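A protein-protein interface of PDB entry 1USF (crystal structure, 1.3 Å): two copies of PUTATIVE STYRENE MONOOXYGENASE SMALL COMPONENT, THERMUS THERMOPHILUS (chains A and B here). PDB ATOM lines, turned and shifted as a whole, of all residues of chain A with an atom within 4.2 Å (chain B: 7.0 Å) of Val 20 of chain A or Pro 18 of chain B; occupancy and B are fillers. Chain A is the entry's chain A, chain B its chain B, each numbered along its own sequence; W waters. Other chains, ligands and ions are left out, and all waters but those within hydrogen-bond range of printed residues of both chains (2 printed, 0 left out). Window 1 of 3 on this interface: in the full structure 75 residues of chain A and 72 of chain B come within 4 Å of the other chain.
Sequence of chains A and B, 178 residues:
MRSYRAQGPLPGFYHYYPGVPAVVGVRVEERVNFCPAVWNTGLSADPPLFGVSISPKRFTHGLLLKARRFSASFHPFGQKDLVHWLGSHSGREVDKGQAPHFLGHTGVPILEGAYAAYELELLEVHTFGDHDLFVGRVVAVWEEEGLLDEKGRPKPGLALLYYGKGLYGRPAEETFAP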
ATOM      1  N   GLY A  19      32.412 -12.440  22.363  1.00  0.00           N
ATOM      2  CA  GLY A  19      31.368 -13.284  22.898  1.00  0.00           C
ATOM      3  C   GLY A  19      31.933 -14.097  24.045  1.00  0.00           C
ATOM      4  O   GLY A  19      33.150 -14.283  24.154  1.00  0.00           O
ATOM      5  N   VAL A  20      31.057 -14.561  24.923  1.00  0.00           N
ATOM      6  CA  VAL A  20      31.489 -15.403  26.023  1.00  0.00           C
ATOM      7  C   VAL A  20      31.654 -16.787  25.415  1.00  0.00           C
ATOM      8  O   VAL A  20      30.769 -17.262  24.699  1.00  0.00           O
ATOM      9  CB  VAL A  20      30.421 -15.478  27.134  1.00  0.00           C
ATOM     10  CG1 VAL A  20      30.791 -16.558  28.140  1.00  0.00           C
ATOM     11  CG2 VAL A  20      30.309 -14.133  27.836  1.00  0.00           C
ATOM     12  N   PRO A  21      32.801 -17.434  25.644  1.00  0.00           N
ATOM     13  CA  PRO A  21      32.993 -18.772  25.084  1.00  0.00           C
ATOM     14  C   PRO A  21      32.416 -19.813  26.036  1.00  0.00           C
ATOM     15  O   PRO A  21      32.642 -19.757  27.246  1.00  0.00           O
ATOM     16  CB  PRO A  21      34.508 -18.876  24.959  1.00  0.00           C
ATOM     17  CG  PRO A  21      34.978 -18.115  26.163  1.00  0.00           C
ATOM     18  CD  PRO A  21      34.065 -16.897  26.182  1.00  0.00           C
ATOM     19  N   ALA A  22      31.643 -20.746  25.500  1.00  0.00           N
ATOM     20  CA  ALA A  22      31.072 -21.799  26.322  1.00  0.00           C
ATOM     21  C   ALA A  22      32.026 -22.983  26.264  1.00  0.00           C
ATOM     22  O   ALA A  22      32.375 -23.441  25.177  1.00  0.00           O
ATOM     23  CB  ALA A  22      29.711 -22.209  25.781  1.00  0.00           C
ATOM     24  N   ASN A  40      27.927 -19.796  20.382  1.00  0.00           N
ATOM     25  CA  ASN A  40      26.912 -20.385  21.244  1.00  0.00           C
ATOM     26  C   ASN A  40      25.828 -19.342  21.438  1.00  0.00           C
ATOM     27  O   ASN A  40      26.075 -18.139  21.301  1.00  0.00           O
ATOM     28  CB  ASN A  40      27.512 -20.813  22.599  1.00  0.00           C
ATOM     29  CG  ASN A  40      27.922 -19.636  23.472  1.00  0.00           C
ATOM     30  OD1 ASN A  40      27.095 -19.039  24.157  1.00  0.00           O
ATOM     31  ND2 ASN A  40      29.204 -19.302  23.447  1.00  0.00           N
ATOM     32  N   ALA A 159      32.988 -12.270  33.600  1.00  0.00           N
ATOM     33  CA  ALA A 159      33.030 -13.101  32.400  1.00  0.00           C
ATOM     34  C   ALA A 159      34.266 -12.975  31.521  1.00  0.00           C
ATOM     35  O   ALA A 159      34.905 -11.926  31.441  1.00  0.00           O
ATOM     36  CB  ALA A 159      31.779 -12.851  31.556  1.00  0.00           C
ATOM     37  N   LEU A 160      34.598 -14.078  30.864  1.00  0.00           N
ATOM     38  CA  LEU A 160      35.714 -14.113  29.938  1.00  0.00           C
ATOM     39  C   LEU A 160      35.112 -13.790  28.575  1.00  0.00           C
ATOM     40  O   LEU A 160      34.092 -14.370  28.191  1.00  0.00           O
ATOM     41  CB  LEU A 160      36.337 -15.511  29.909  1.00  0.00           C
ATOM     42  CG  LEU A 160      37.417 -15.759  28.855  1.00  0.00           C
ATOM     43  CD1 LEU A 160      38.610 -14.843  29.104  1.00  0.00           C
ATOM     44  CD2 LEU A 160      37.841 -17.221  28.909  1.00  0.00           C
ATOM     45  N   LEU A 161      35.715 -12.853  27.855  1.00  0.00           N
ATOM     46  CA  LEU A 161      35.229 -12.489  26.529  1.00  0.00           C
ATOM     47  C   LEU A 161      36.267 -12.900  25.496  1.00  0.00           C
ATOM     48  O   LEU A 161      37.468 -12.757  25.730  1.00  0.00           O
ATOM     49  CB  LEU A 161      35.003 -10.976  26.429  1.00  0.00           C
ATOM     50  CG  LEU A 161      33.908 -10.365  27.305  1.00  0.00           C
ATOM     51  CD1 LEU A 161      33.862  -8.860  27.095  1.00  0.00           C
ATOM     52  CD2 LEU A 161      32.571 -10.989  26.951  1.00  0.00           C
ATOM     53  N   PRO A 171      34.409  -7.918  30.634  1.00  0.00           N
ATOM     54  CA  PRO A 171      33.555  -6.731  30.613  1.00  0.00           C
ATOM     55  C   PRO A 171      34.080  -5.710  31.611  1.00  0.00           C
ATOM     56  O   PRO A 171      34.792  -6.060  32.561  1.00  0.00           O
ATOM     57  CB  PRO A 171      32.190  -7.260  31.057  1.00  0.00           C
ATOM     58  CG  PRO A 171      32.266  -8.744  30.829  1.00  0.00           C
ATOM     59  CD  PRO A 171      33.689  -9.075  31.184  1.00  0.00           C
ATOM     60  N   TYR B  14      20.496 -16.515  32.167  1.00  0.00           N
ATOM     61  CA  TYR B  14      21.553 -15.576  31.811  1.00  0.00           C
ATOM     62  C   TYR B  14      22.974 -16.022  32.132  1.00  0.00           C
ATOM     63  O   TYR B  14      23.897 -15.207  32.107  1.00  0.00           O
ATOM     64  CB  TYR B  14      21.298 -14.245  32.526  1.00  0.00           C
ATOM     65  CG  TYR B  14      19.921 -13.685  32.297  1.00  0.00           C
ATOM     66  CD1 TYR B  14      18.971 -13.664  33.318  1.00  0.00           C
ATOM     67  CD2 TYR B  14      19.557 -13.194  31.048  1.00  0.00           C
ATOM     68  CE1 TYR B  14      17.684 -13.165  33.091  1.00  0.00           C
ATOM     69  CE2 TYR B  14      18.284 -12.698  30.809  1.00  0.00           C
ATOM     70  CZ  TYR B  14      17.355 -12.688  31.831  1.00  0.00           C
ATOM     71  OH  TYR B  14      16.095 -12.203  31.582  1.00  0.00           O
ATOM     72  N   HIS B  15      23.166 -17.302  32.409  1.00  0.00           N
ATOM     73  CA  HIS B  15      24.488 -17.793  32.779  1.00  0.00           C
ATOM     74  C   HIS B  15      25.559 -17.587  31.720  1.00  0.00           C
ATOM     75  O   HIS B  15      26.754 -17.506  32.041  1.00  0.00           O
ATOM     76  CB  HIS B  15      24.399 -19.273  33.142  1.00  0.00           C
ATOM     77  CG  HIS B  15      23.309 -19.578  34.117  1.00  0.00           C
ATOM     78  ND1 HIS B  15      21.993 -19.723  33.735  1.00  0.00           N
ATOM     79  CD2 HIS B  15      23.329 -19.714  35.464  1.00  0.00           C
ATOM     80  CE1 HIS B  15      21.248 -19.936  34.806  1.00  0.00           C
ATOM     81  NE2 HIS B  15      22.033 -19.934  35.869  1.00  0.00           N
ATOM     82  N   TYR B  16      25.122 -17.494  30.466  1.00  0.00           N
ATOM     83  CA  TYR B  16      26.021 -17.316  29.334  1.00  0.00           C
ATOM     84  C   TYR B  16      26.116 -15.877  28.832  1.00  0.00           C
ATOM     85  O   TYR B  16      26.729 -15.622  27.797  1.00  0.00           O
ATOM     86  CB  TYR B  16      25.602 -18.238  28.182  1.00  0.00           C
ATOM     87  CG  TYR B  16      24.144 -18.115  27.811  1.00  0.00           C
ATOM     88  CD1 TYR B  16      23.161 -18.774  28.545  1.00  0.00           C
ATOM     89  CD2 TYR B  16      23.742 -17.305  26.749  1.00  0.00           C
ATOM     90  CE1 TYR B  16      21.808 -18.628  28.239  1.00  0.00           C
ATOM     91  CE2 TYR B  16      22.394 -17.149  26.435  1.00  0.00           C
ATOM     92  CZ  TYR B  16      21.432 -17.811  27.184  1.00  0.00           C
ATOM     93  OH  TYR B  16      20.097 -17.627  26.899  1.00  0.00           O
ATOM     94  N   TYR B  17      25.500 -14.944  29.555  1.00  0.00           N
ATOM     95  CA  TYR B  17      25.558 -13.529  29.194  1.00  0.00           C
ATOM     96  C   TYR B  17      26.841 -12.962  29.821  1.00  0.00           C
ATOM     97  O   TYR B  17      27.430 -13.580  30.705  1.00  0.00           O
ATOM     98  CB  TYR B  17      24.338 -12.783  29.750  1.00  0.00           C
ATOM     99  CG  TYR B  17      23.042 -12.956  28.974  1.00  0.00           C
ATOM    100  CD1 TYR B  17      22.517 -14.221  28.708  1.00  0.00           C
ATOM    101  CD2 TYR B  17      22.296 -11.841  28.586  1.00  0.00           C
ATOM    102  CE1 TYR B  17      21.274 -14.370  28.084  1.00  0.00           C
ATOM    103  CE2 TYR B  17      21.055 -11.982  27.966  1.00  0.00           C
ATOM    104  CZ  TYR B  17      20.546 -13.248  27.723  1.00  0.00           C
ATOM    105  OH  TYR B  17      19.291 -13.382  27.155  1.00  0.00           O
ATOM    106  N   PRO B  18      27.275 -11.766  29.401  1.00  0.00           N
ATOM    107  CA  PRO B  18      26.670 -10.893  28.399  1.00  0.00           C
ATOM    108  C   PRO B  18      26.968 -11.305  26.970  1.00  0.00           C
ATOM    109  O   PRO B  18      27.821 -12.155  26.705  1.00  0.00           O
ATOM    110  CB  PRO B  18      27.293  -9.542  28.715  1.00  0.00           C
ATOM    111  CG  PRO B  18      28.699  -9.942  29.041  1.00  0.00           C
ATOM    112  CD  PRO B  18      28.512 -11.162  29.932  1.00  0.00           C
ATOM    113  N   GLY B  19      26.255 -10.668  26.053  1.00  0.00           N
ATOM    114  CA  GLY B  19      26.457 -10.918  24.645  1.00  0.00           C
ATOM    115  C   GLY B  19      26.237  -9.629  23.889  1.00  0.00           C
ATOM    116  O   GLY B  19      25.584  -8.710  24.389  1.00  0.00           O
ATOM    117  N   VAL B  20      26.808  -9.542  22.694  1.00  0.00           N
ATOM    118  CA  VAL B  20      26.614  -8.364  21.865  1.00  0.00           C
ATOM    119  C   VAL B  20      25.238  -8.527  21.236  1.00  0.00           C
ATOM    120  O   VAL B  20      24.914  -9.594  20.712  1.00  0.00           O
ATOM    121  CB  VAL B  20      27.661  -8.284  20.736  1.00  0.00           C
ATOM    122  CG1 VAL B  20      27.285  -7.177  19.754  1.00  0.00           C
ATOM    123  CG2 VAL B  20      29.033  -8.007  21.316  1.00  0.00           C
ATOM    124  N   VAL B  38      19.923 -10.616  21.258  1.00  0.00           N
ATOM    125  CA  VAL B  38      21.139 -11.033  21.938  1.00  0.00           C
ATOM    126  C   VAL B  38      21.393 -12.512  21.661  1.00  0.00           C
ATOM    127  O   VAL B  38      22.505 -13.006  21.827  1.00  0.00           O
ATOM    128  CB  VAL B  38      21.068 -10.757  23.466  1.00  0.00           C
ATOM    129  CG1 VAL B  38      20.039 -11.653  24.130  1.00  0.00           C
ATOM    130  CG2 VAL B  38      22.445 -10.939  24.089  1.00  0.00           C
ATOM    131  N   LEU B 161      27.386  -4.384  25.251  1.00  0.00           N
ATOM    132  CA  LEU B 161      27.130  -5.705  25.819  1.00  0.00           C
ATOM    133  C   LEU B 161      25.793  -5.691  26.536  1.00  0.00           C
ATOM    134  O   LEU B 161      25.426  -4.696  27.161  1.00  0.00           O
ATOM    135  CB  LEU B 161      28.224  -6.083  26.816  1.00  0.00           C
ATOM    136  CG  LEU B 161      29.641  -6.216  26.257  1.00  0.00           C
ATOM    137  CD1 LEU B 161      30.591  -6.549  27.395  1.00  0.00           C
ATOM    138  CD2 LEU B 161      29.681  -7.300  25.182  1.00  0.00           C
ATOM    139  N   TYR B 162      25.053  -6.788  26.437  1.00  0.00           N
ATOM    140  CA  TYR B 162      23.766  -6.891  27.107  1.00  0.00           C
ATOM    141  C   TYR B 162      23.833  -8.016  28.128  1.00  0.00           C
ATOM    142  O   TYR B 162      24.223  -9.136  27.799  1.00  0.00           O
ATOM    143  CB  TYR B 162      22.660  -7.179  26.096  1.00  0.00           C
ATOM    144  CG  TYR B 162      21.276  -7.210  26.705  1.00  0.00           C
ATOM    145  CD1 TYR B 162      20.791  -6.125  27.434  1.00  0.00           C
ATOM    146  CD2 TYR B 162      20.430  -8.310  26.512  1.00  0.00           C
ATOM    147  CE1 TYR B 162      19.498  -6.126  27.950  1.00  0.00           C
ATOM    148  CE2 TYR B 162      19.134  -8.323  27.027  1.00  0.00           C
ATOM    149  CZ  TYR B 162      18.674  -7.223  27.743  1.00  0.00           C
ATOM    150  OH  TYR B 162      17.394  -7.208  28.251  1.00  0.00           O
ATOM    151  N   TYR B 163      23.464  -7.704  29.371  1.00  0.00           N
ATOM    152  CA  TYR B 163      23.483  -8.669  30.474  1.00  0.00           C
ATOM    153  C   TYR B 163      22.132  -9.318  30.744  1.00  0.00           C
ATOM    154  O   TYR B 163      22.048 -10.258  31.533  1.00  0.00           O
ATOM    155  CB  TYR B 163      23.923  -7.978  31.764  1.00  0.00           C
ATOM    156  CG  TYR B 163      25.369  -7.580  31.818  1.00  0.00           C
ATOM    157  CD1 TYR B 163      26.362  -8.513  32.099  1.00  0.00           C
ATOM    158  CD2 TYR B 163      25.744  -6.252  31.629  1.00  0.00           C
ATOM    159  CE1 TYR B 163      27.699  -8.130  32.199  1.00  0.00           C
ATOM    160  CE2 TYR B 163      27.070  -5.859  31.725  1.00  0.00           C
ATOM    161  CZ  TYR B 163      28.041  -6.800  32.012  1.00  0.00           C
ATOM    162  OH  TYR B 163      29.350  -6.393  32.132  1.00  0.00           O
ATOM    163  N   GLY B 164      21.082  -8.806  30.109  1.00  0.00           N
ATOM    164  CA  GLY B 164      19.751  -9.338  30.337  1.00  0.00           C
ATOM    165  C   GLY B 164      18.945  -8.407  31.225  1.00  0.00           C
ATOM    166  O   GLY B 164      19.506  -7.634  31.999  1.00  0.00           O
ATOM    167  N   LEU B 167      19.872  -4.511  31.385  1.00  0.00           N
ATOM    168  CA  LEU B 167      21.162  -4.068  31.900  1.00  0.00           C
ATOM    169  C   LEU B 167      22.214  -4.217  30.811  1.00  0.00           C
ATOM    170  O   LEU B 167      22.330  -5.281  30.200  1.00  0.00           O
ATOM    171  CB  LEU B 167      21.555  -4.901  33.122  1.00  0.00           C
ATOM    172  CG  LEU B 167      22.800  -4.448  33.887  1.00  0.00           C
ATOM    173  CD1 LEU B 167      22.542  -3.105  34.571  1.00  0.00           C
ATOM    174  CD2 LEU B 167      23.166  -5.513  34.914  1.00  0.00           C
ATOM    175  N   GLY B 169      26.392  -3.078  29.274  1.00  0.00           N
ATOM    176  CA  GLY B 169      27.752  -2.789  29.665  1.00  0.00           C
ATOM    177  C   GLY B 169      28.611  -2.640  28.430  1.00  0.00           C
ATOM    178  O   GLY B 169      28.103  -2.412  27.332  1.00  0.00           O
HETATM  179  O   HOH W   1      27.129 -16.497  25.211  1.00  0.00           O
HETATM  180  O   HOH W   2      28.285 -13.947  24.551  1.00  0.00           O
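The backbone carbonyl oxygen (O) of Val 20 of chain A is in hydrogen-bond range of the side-chain amide nitrogen (ND2) of Asn 40 of chain A (2.9 Å).
Tyr 16 of chain B touches Val 20 of chain A (O to CB, 3.8 Å).
Val 20 of chain A touches Pro 18 of chain B.
Tyr 163 of chain B touches Pro 171 of chain A (OH to CB, 3.2 Å).
Printed residues of chain B within 4 Å of Val 20 of chain A: Tyr 16 (3.8 Å) and Pro 18 (3.4 Å).
Printed residues of chain B within 4 Å of Pro 171 of chain A: Tyr 163 (3.2 Å).
Printed residues of chain A within 4 Å of Tyr 16 of chain B: Val 20 (3.8 Å).
Pro 18 of chain B touches just one residue of chain A: Val 20 (3.4 Å).
Tyr 162 of chain B touches none of the printed residues of chain A.
Of the printed residues of chain A, Tyr 163 of chain B touches Pro 171.
The nearest residue of chain B that does not touch Val 20 of chain A is Tyr 17 of chain B (4.1 Å).
The nearest residue of chain A that does not touch Pro 18 of chain B is Ala 159 of chain A (4.02 Å).
Of the 14 printed residues of chain B, 3 touch a printed residue of chain A.
Hydrophobic or aromatic side chains of chain B within 4 Å of the printed part of chain A: Tyr 163.
Of the 9 printed residues of chain A, 2 touch a printed residue of chain B.
Hydrophobic or aromatic side chains of chain A within 4 Å of the printed part of chain B: Val 20 and Pro 171.
Among the printed residues, 3 pairs touch across the chains.
Among the printed residues, no Asp or Glu carboxylate lies within 4 Å of a Lys or Arg side-chain nitrogen of the other chain.
Positions printed for both chains: 19, 20 and 161.
Of the 3 pairs that touch across the chains among the printed residues, none has its exchanged pair printed and touching as well.
Water W1 bridges OD1 of Asn 40 of chain A (2.8 Å) and O of Tyr 16 of chain B (2.8 Å).
Water W2 lies within hydrogen-bond range of the backbone carbonyl oxygen (O) of Pro 18 of chain B (2.8 Å) and the backbone NH (N) of Val 20 of chain A (2.9 Å).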
